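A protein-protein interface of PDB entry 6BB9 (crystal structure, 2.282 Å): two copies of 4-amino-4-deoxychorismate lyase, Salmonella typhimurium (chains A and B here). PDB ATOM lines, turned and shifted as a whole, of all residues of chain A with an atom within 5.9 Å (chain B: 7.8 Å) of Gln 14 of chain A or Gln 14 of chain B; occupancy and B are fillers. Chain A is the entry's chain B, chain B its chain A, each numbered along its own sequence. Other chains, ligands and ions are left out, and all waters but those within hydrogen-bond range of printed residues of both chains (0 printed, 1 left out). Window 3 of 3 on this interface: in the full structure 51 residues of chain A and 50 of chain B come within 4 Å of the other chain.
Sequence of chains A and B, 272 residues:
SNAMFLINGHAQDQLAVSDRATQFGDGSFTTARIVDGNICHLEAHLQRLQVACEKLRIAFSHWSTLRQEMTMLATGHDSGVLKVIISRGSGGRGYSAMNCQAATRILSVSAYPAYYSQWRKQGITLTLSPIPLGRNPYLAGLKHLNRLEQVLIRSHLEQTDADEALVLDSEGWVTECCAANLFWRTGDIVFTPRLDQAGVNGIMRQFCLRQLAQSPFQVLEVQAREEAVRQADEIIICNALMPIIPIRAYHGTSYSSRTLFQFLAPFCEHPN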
ATOM      1  N   ILE A   7     -21.338 -19.416   9.327  1.00  0.00           N
ATOM      2  CA  ILE A   7     -21.522 -20.814   9.694  1.00  0.00           C
ATOM      3  C   ILE A   7     -20.146 -21.410   9.939  1.00  0.00           C
ATOM      4  O   ILE A   7     -19.364 -21.587   8.996  1.00  0.00           O
ATOM      5  CB  ILE A   7     -22.275 -21.588   8.607  1.00  0.00           C
ATOM      6  CG1 ILE A   7     -23.601 -20.889   8.302  1.00  0.00           C
ATOM      7  CG2 ILE A   7     -22.491 -23.029   9.039  1.00  0.00           C
ATOM      8  CD1 ILE A   7     -24.433 -21.580   7.256  1.00  0.00           C
ATOM      9  N   GLN A  12     -21.469 -17.506   4.552  1.00  0.00           N
ATOM     10  CA  GLN A  12     -22.121 -18.592   3.838  1.00  0.00           C
ATOM     11  C   GLN A  12     -23.611 -18.565   4.142  1.00  0.00           C
ATOM     12  O   GLN A  12     -23.994 -18.488   5.311  1.00  0.00           O
ATOM     13  CB  GLN A  12     -21.487 -19.915   4.272  1.00  0.00           C
ATOM     14  CG  GLN A  12     -22.045 -21.172   3.665  1.00  0.00           C
ATOM     15  CD  GLN A  12     -21.371 -22.401   4.251  1.00  0.00           C
ATOM     16  OE1 GLN A  12     -20.309 -22.296   4.868  1.00  0.00           O
ATOM     17  NE2 GLN A  12     -21.987 -23.565   4.073  1.00  0.00           N
ATOM     18  N   ASP A  13     -24.470 -18.609   3.122  1.00  0.00           N
ATOM     19  CA  ASP A  13     -25.908 -18.567   3.368  1.00  0.00           C
ATOM     20  C   ASP A  13     -26.605 -19.884   3.023  1.00  0.00           C
ATOM     21  O   ASP A  13     -27.817 -19.899   2.791  1.00  0.00           O
ATOM     22  CB  ASP A  13     -26.545 -17.402   2.610  1.00  0.00           C
ATOM     23  CG  ASP A  13     -26.115 -17.347   1.173  1.00  0.00           C
ATOM     24  OD1 ASP A  13     -25.459 -18.308   0.717  1.00  0.00           O
ATOM     25  OD2 ASP A  13     -26.426 -16.340   0.500  1.00  0.00           O
ATOM     26  N   GLN A  14     -25.869 -20.994   3.022  1.00  0.00           N
ATOM     27  CA  GLN A  14     -26.447 -22.304   2.776  1.00  0.00           C
ATOM     28  C   GLN A  14     -25.793 -23.323   3.694  1.00  0.00           C
ATOM     29  O   GLN A  14     -24.600 -23.229   3.985  1.00  0.00           O
ATOM     30  CB  GLN A  14     -26.273 -22.731   1.320  1.00  0.00           C
ATOM     31  CG  GLN A  14     -27.232 -22.082   0.353  1.00  0.00           C
ATOM     32  CD  GLN A  14     -27.247 -22.806  -0.973  1.00  0.00           C
ATOM     33  OE1 GLN A  14     -26.195 -23.100  -1.539  1.00  0.00           O
ATOM     34  NE2 GLN A  14     -28.441 -23.127  -1.465  1.00  0.00           N
ATOM     35  N   LEU A  15     -26.580 -24.294   4.148  1.00  0.00           N
ATOM     36  CA  LEU A  15     -26.124 -25.321   5.070  1.00  0.00           C
ATOM     37  C   LEU A  15     -26.416 -26.704   4.498  1.00  0.00           C
ATOM     38  O   LEU A  15     -27.409 -26.901   3.793  1.00  0.00           O
ATOM     39  CB  LEU A  15     -26.807 -25.157   6.428  1.00  0.00           C
ATOM     40  CG  LEU A  15     -26.608 -26.253   7.474  1.00  0.00           C
ATOM     41  CD1 LEU A  15     -25.156 -26.311   7.946  1.00  0.00           C
ATOM     42  CD2 LEU A  15     -27.563 -26.041   8.646  1.00  0.00           C
ATOM     43  N   ALA A  16     -25.542 -27.663   4.804  1.00  0.00           N
ATOM     44  CA  ALA A  16     -25.737 -29.033   4.340  1.00  0.00           C
ATOM     45  C   ALA A  16     -27.115 -29.542   4.744  1.00  0.00           C
ATOM     46  O   ALA A  16     -27.540 -29.372   5.891  1.00  0.00           O
ATOM     47  CB  ALA A  16     -24.645 -29.942   4.906  1.00  0.00           C
ATOM     48  N   VAL A  17     -27.816 -30.158   3.783  1.00  0.00           N
ATOM     49  CA  VAL A  17     -29.195 -30.599   4.007  1.00  0.00           C
ATOM     50  C   VAL A  17     -29.261 -31.619   5.129  1.00  0.00           C
ATOM     51  O   VAL A  17     -30.249 -31.683   5.872  1.00  0.00           O
ATOM     52  CB  VAL A  17     -29.795 -31.181   2.707  1.00  0.00           C
ATOM     53  CG1 VAL A  17     -31.312 -31.292   2.816  1.00  0.00           C
ATOM     54  CG2 VAL A  17     -29.408 -30.339   1.522  1.00  0.00           C
ATOM     55  N   ALA B   3     -23.147 -36.462  -0.487  1.00  0.00           N
ATOM     56  CA  ALA B   3     -24.532 -36.534  -0.032  1.00  0.00           C
ATOM     57  C   ALA B   3     -25.440 -35.611  -0.849  1.00  0.00           C
ATOM     58  O   ALA B   3     -25.529 -34.420  -0.556  1.00  0.00           O
ATOM     59  CB  ALA B   3     -24.620 -36.179   1.452  1.00  0.00           C
ATOM     60  N   MET B   4     -26.130 -36.165  -1.849  1.00  0.00           N
ATOM     61  CA  MET B   4     -26.888 -35.375  -2.811  1.00  0.00           C
ATOM     62  C   MET B   4     -28.392 -35.609  -2.673  1.00  0.00           C
ATOM     63  O   MET B   4     -28.856 -36.750  -2.555  1.00  0.00           O
ATOM     64  CB  MET B   4     -26.439 -35.693  -4.238  1.00  0.00           C
ATOM     65  CG  MET B   4     -26.500 -34.521  -5.228  1.00  0.00           C
ATOM     66  SD  MET B   4     -25.122 -33.365  -5.094  1.00  0.00           S
ATOM     67  CE  MET B   4     -25.383 -32.322  -6.529  1.00  0.00           C
ATOM     68  N   PHE B   5     -29.145 -34.512  -2.719  1.00  0.00           N
ATOM     69  CA  PHE B   5     -30.585 -34.454  -2.526  1.00  0.00           C
ATOM     70  C   PHE B   5     -31.241 -33.843  -3.770  1.00  0.00           C
ATOM     71  O   PHE B   5     -30.572 -33.296  -4.651  1.00  0.00           O
ATOM     72  CB  PHE B   5     -30.917 -33.627  -1.275  1.00  0.00           C
ATOM     73  CG  PHE B   5     -30.393 -34.212   0.018  1.00  0.00           C
ATOM     74  CD1 PHE B   5     -29.031 -34.252   0.291  1.00  0.00           C
ATOM     75  CD2 PHE B   5     -31.273 -34.699   0.975  1.00  0.00           C
ATOM     76  CE1 PHE B   5     -28.552 -34.790   1.478  1.00  0.00           C
ATOM     77  CE2 PHE B   5     -30.800 -35.235   2.166  1.00  0.00           C
ATOM     78  CZ  PHE B   5     -29.439 -35.279   2.416  1.00  0.00           C
ATOM     79  N   ILE B   7     -33.829 -30.858  -4.179  1.00  0.00           N
ATOM     80  CA  ILE B   7     -34.459 -29.768  -3.442  1.00  0.00           C
ATOM     81  C   ILE B   7     -35.198 -28.903  -4.450  1.00  0.00           C
ATOM     82  O   ILE B   7     -34.579 -28.284  -5.324  1.00  0.00           O
ATOM     83  CB  ILE B   7     -33.436 -28.948  -2.646  1.00  0.00           C
ATOM     84  CG1 ILE B   7     -32.841 -29.797  -1.525  1.00  0.00           C
ATOM     85  CG2 ILE B   7     -34.070 -27.683  -2.073  1.00  0.00           C
ATOM     86  CD1 ILE B   7     -31.745 -29.090  -0.782  1.00  0.00           C
ATOM     87  N   HIS B  10     -34.154 -29.634  -7.836  1.00  0.00           N
ATOM     88  CA  HIS B  10     -32.779 -29.328  -8.202  1.00  0.00           C
ATOM     89  C   HIS B  10     -31.829 -30.177  -7.363  1.00  0.00           C
ATOM     90  O   HIS B  10     -31.970 -30.250  -6.138  1.00  0.00           O
ATOM     91  CB  HIS B  10     -32.487 -27.834  -8.007  1.00  0.00           C
ATOM     92  CG  HIS B  10     -31.312 -27.340  -8.791  1.00  0.00           C
ATOM     93  ND1 HIS B  10     -30.101 -27.035  -8.206  1.00  0.00           N
ATOM     94  CD2 HIS B  10     -31.161 -27.098 -10.115  1.00  0.00           C
ATOM     95  CE1 HIS B  10     -29.255 -26.626  -9.136  1.00  0.00           C
ATOM     96  NE2 HIS B  10     -29.873 -26.656 -10.304  1.00  0.00           N
ATOM     97  N   ALA B  11     -30.861 -30.806  -8.031  1.00  0.00           N
ATOM     98  CA  ALA B  11     -29.876 -31.682  -7.396  1.00  0.00           C
ATOM     99  C   ALA B  11     -28.860 -30.842  -6.626  1.00  0.00           C
ATOM    100  O   ALA B  11     -27.967 -30.236  -7.220  1.00  0.00           O
ATOM    101  CB  ALA B  11     -29.188 -32.537  -8.452  1.00  0.00           C
ATOM    102  N   GLN B  12     -28.981 -30.822  -5.295  1.00  0.00           N
ATOM    103  CA  GLN B  12     -28.139 -30.008  -4.420  1.00  0.00           C
ATOM    104  C   GLN B  12     -27.813 -30.779  -3.149  1.00  0.00           C
ATOM    105  O   GLN B  12     -28.551 -31.672  -2.732  1.00  0.00           O
ATOM    106  CB  GLN B  12     -28.812 -28.693  -3.989  1.00  0.00           C
ATOM    107  CG  GLN B  12     -29.370 -27.820  -5.080  1.00  0.00           C
ATOM    108  CD  GLN B  12     -30.365 -26.807  -4.538  1.00  0.00           C
ATOM    109  OE1 GLN B  12     -31.167 -26.251  -5.286  1.00  0.00           O
ATOM    110  NE2 GLN B  12     -30.316 -26.562  -3.233  1.00  0.00           N
ATOM    111  N   ASP B  13     -26.716 -30.387  -2.502  1.00  0.00           N
ATOM    112  CA  ASP B  13     -26.349 -30.908  -1.190  1.00  0.00           C
ATOM    113  C   ASP B  13     -26.535 -29.886  -0.074  1.00  0.00           C
ATOM    114  O   ASP B  13     -26.258 -30.202   1.092  1.00  0.00           O
ATOM    115  CB  ASP B  13     -24.897 -31.415  -1.194  1.00  0.00           C
ATOM    116  CG  ASP B  13     -23.926 -30.422  -1.809  1.00  0.00           C
ATOM    117  OD1 ASP B  13     -24.337 -29.278  -2.104  1.00  0.00           O
ATOM    118  OD2 ASP B  13     -22.745 -30.789  -2.006  1.00  0.00           O
ATOM    119  N   GLN B  14     -27.010 -28.680  -0.392  1.00  0.00           N
ATOM    120  CA  GLN B  14     -27.162 -27.618   0.588  1.00  0.00           C
ATOM    121  C   GLN B  14     -28.538 -26.985   0.455  1.00  0.00           C
ATOM    122  O   GLN B  14     -29.195 -27.074  -0.584  1.00  0.00           O
ATOM    123  CB  GLN B  14     -26.071 -26.547   0.445  1.00  0.00           C
ATOM    124  CG  GLN B  14     -24.676 -27.048   0.795  1.00  0.00           C
ATOM    125  CD  GLN B  14     -23.659 -25.930   0.874  1.00  0.00           C
ATOM    126  OE1 GLN B  14     -23.542 -25.116  -0.041  1.00  0.00           O
ATOM    127  NE2 GLN B  14     -22.922 -25.876   1.983  1.00  0.00           N
ATOM    128  N   LEU B  15     -28.963 -26.350   1.538  1.00  0.00           N
ATOM    129  CA  LEU B  15     -30.249 -25.683   1.645  1.00  0.00           C
ATOM    130  C   LEU B  15     -30.033 -24.305   2.254  1.00  0.00           C
ATOM    131  O   LEU B  15     -29.149 -24.119   3.093  1.00  0.00           O
ATOM    132  CB  LEU B  15     -31.216 -26.503   2.518  1.00  0.00           C
ATOM    133  CG  LEU B  15     -32.611 -25.957   2.829  1.00  0.00           C
ATOM    134  CD1 LEU B  15     -33.453 -25.822   1.564  1.00  0.00           C
ATOM    135  CD2 LEU B  15     -33.291 -26.878   3.813  1.00  0.00           C
ATOM    136  N   ALA B  16     -30.840 -23.336   1.823  1.00  0.00           N
ATOM    137  CA  ALA B  16     -30.763 -21.998   2.404  1.00  0.00           C
ATOM    138  C   ALA B  16     -30.944 -22.057   3.919  1.00  0.00           C
ATOM    139  O   ALA B  16     -31.860 -22.711   4.425  1.00  0.00           O
ATOM    140  CB  ALA B  16     -31.820 -21.094   1.779  1.00  0.00           C
ATOM    141  N   VAL B  17     -30.055 -21.378   4.648  1.00  0.00           N
ATOM    142  CA  VAL B  17     -30.124 -21.398   6.104  1.00  0.00           C
ATOM    143  C   VAL B  17     -31.426 -20.787   6.587  1.00  0.00           C
ATOM    144  O   VAL B  17     -31.944 -21.166   7.641  1.00  0.00           O
ATOM    145  CB  VAL B  17     -28.911 -20.676   6.711  1.00  0.00           C
ATOM    146  CG1 VAL B  17     -28.839 -20.933   8.198  1.00  0.00           C
ATOM    147  CG2 VAL B  17     -27.658 -21.146   6.041  1.00  0.00           C
ATOM    148  N   SER B  18     -31.990 -19.854   5.823  1.00  0.00           N
ATOM    149  CA  SER B  18     -33.243 -19.222   6.221  1.00  0.00           C
ATOM    150  C   SER B  18     -34.415 -20.196   6.299  1.00  0.00           C
ATOM    151  O   SER B  18     -35.443 -19.828   6.878  1.00  0.00           O
ATOM    152  CB  SER B  18     -33.592 -18.104   5.239  1.00  0.00           C
ATOM    153  OG  SER B  18     -33.821 -18.649   3.953  1.00  0.00           O
ATOM    154  N   ILE B 106     -37.827 -31.649  -0.106  1.00  0.00           N
ATOM    155  CA  ILE B 106     -36.498 -32.239  -0.042  1.00  0.00           C
ATOM    156  C   ILE B 106     -36.642 -33.749  -0.157  1.00  0.00           C
ATOM    157  O   ILE B 106     -37.385 -34.366   0.612  1.00  0.00           O
ATOM    158  CB  ILE B 106     -35.770 -31.863   1.258  1.00  0.00           C
ATOM    159  CG1 ILE B 106     -35.596 -30.344   1.343  1.00  0.00           C
ATOM    160  CG2 ILE B 106     -34.444 -32.588   1.346  1.00  0.00           C
ATOM    161  CD1 ILE B 106     -35.106 -29.859   2.698  1.00  0.00           C
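Ala 16 of chain B touches Asp 13 of chain A. Gln 14 of chain A touches Gln 14 of chain B. Leu 15 of chain B touches Gln 14 of chain A. Val 17 of chain B touches Gln 14 of chain A (CG2 to N, 3.5 Å). CG2 of Val 17 of chain B touches N of Leu 15 of chain A (3.8 Å). CA of Ala 16 of chain A touches O of Asp 13 of chain B, at 3.5 Å. CD2 of Phe 5 of chain B touches CG1 of Val 17 of chain A, at 3.9 Å. CD1 of Ile 7 of chain B touches CG2 of Val 17 of chain A, 3.5 Å away. Val 17 of chain A touches Gln 14 of chain B (CG2 to N, 3.5 Å). CG1 of Val 17 of chain A touches CG2 of Ile 106 of chain B (3.7 Å).
Printed residues of chain B that touch a printed residue of chain A: Phe 5, Ile 7, Asp 13, Gln 14, Leu 15, Ala 16, Val 17 and Ile 106. Of the 7 printed residues of chain A, 7 touch a printed residue of chain B. Hydrophobic or aromatic side chains of chain A within 4 Å of the printed part of chain B: Ile 7 and Val 17. Among the printed residues, 16 pairs touch across the chains. Among the printed residues, no Asp or Glu carboxylate lies within 4 Å of a Lys or Arg side-chain nitrogen of the other chain.
The backbone carbonyl oxygen of Asp 13 of chain A is in hydrogen-bond range of the backbone NH of Val 17 of chain B (3.3 Å). N of Leu 15 of chain A sits at hydrogen-bond distance from O of Leu 15 of chain B, at 2.8 Å. NE2 of Gln 14 of chain B lies close to NE2 of Gln 12 of chain A (3.3 Å). O of Asp 13 of chain B is in hydrogen-bond range of N of Val 17 of chain A, at 3.1 Å.
Ile 7 of chain A touches Val 17 of chain B, and with the chains exchanged Val 17 of chain A touches Ile 7 of chain B. Gln 12 of chain A touches Gln 14 of chain B, but with the chains exchanged Gln 14 of chain A does not touch Gln 12 of chain B (4.3 Å). Asp 13 of chain A touches Val 17 of chain B, and with the chains exchanged Val 17 of chain A touches Asp 13 of chain B. Gln 14 of chain A touches Leu 15 of chain B, and with the chains exchanged Leu 15 of chain A touches Gln 14 of chain B. Positions printed for both chains: 7, 12, 13, 14, 15, 16 and 17.
The backbone carbonyl oxygen (O) of Gln 14 of chain A is in hydrogen-bond range of the side-chain amide nitrogen (NE2) of Gln 12 of chain A. O of Gln 12 of chain B sits at hydrogen-bond distance from N of Phe 5 of chain B (2.9 Å). NE2 of Gln 12 of chain B is in hydrogen-bond range of O of Gln 14 of chain B (2.9 Å).
Of chain B, only Gln 14, Leu 15 and Val 17 come within 4 Å of Gln 14 of chain A. Of the printed residues of chain B, Leu 15 of chain A touches Gln 14, Leu 15 and Val 17. Met 4 of chain B touches none of the printed residues of chain A. Gln 12 of chain B touches none of the printed residues of chain A. Of chain A, only Gln 12, Gln 14, Leu 15 and Val 17 come within 4 Å of Gln 14 of chain B. Of the printed residues of chain A, Ala 16 of chain B touches Asp 13 (3.6 Å). Of the printed residues of chain A, Val 17 of chain B touches Ile 7 (3.5 Å), Asp 13 (3.3 Å), Gln 14 (3.5 Å) and Leu 15 (3.8 Å). The nearest residue of chain B that does not touch Gln 14 of chain A is Ala 16 of chain B (4.1 Å). The nearest residue of chain A that does not touch Gln 14 of chain B is Ala 16 of chain A (4.1 Å).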
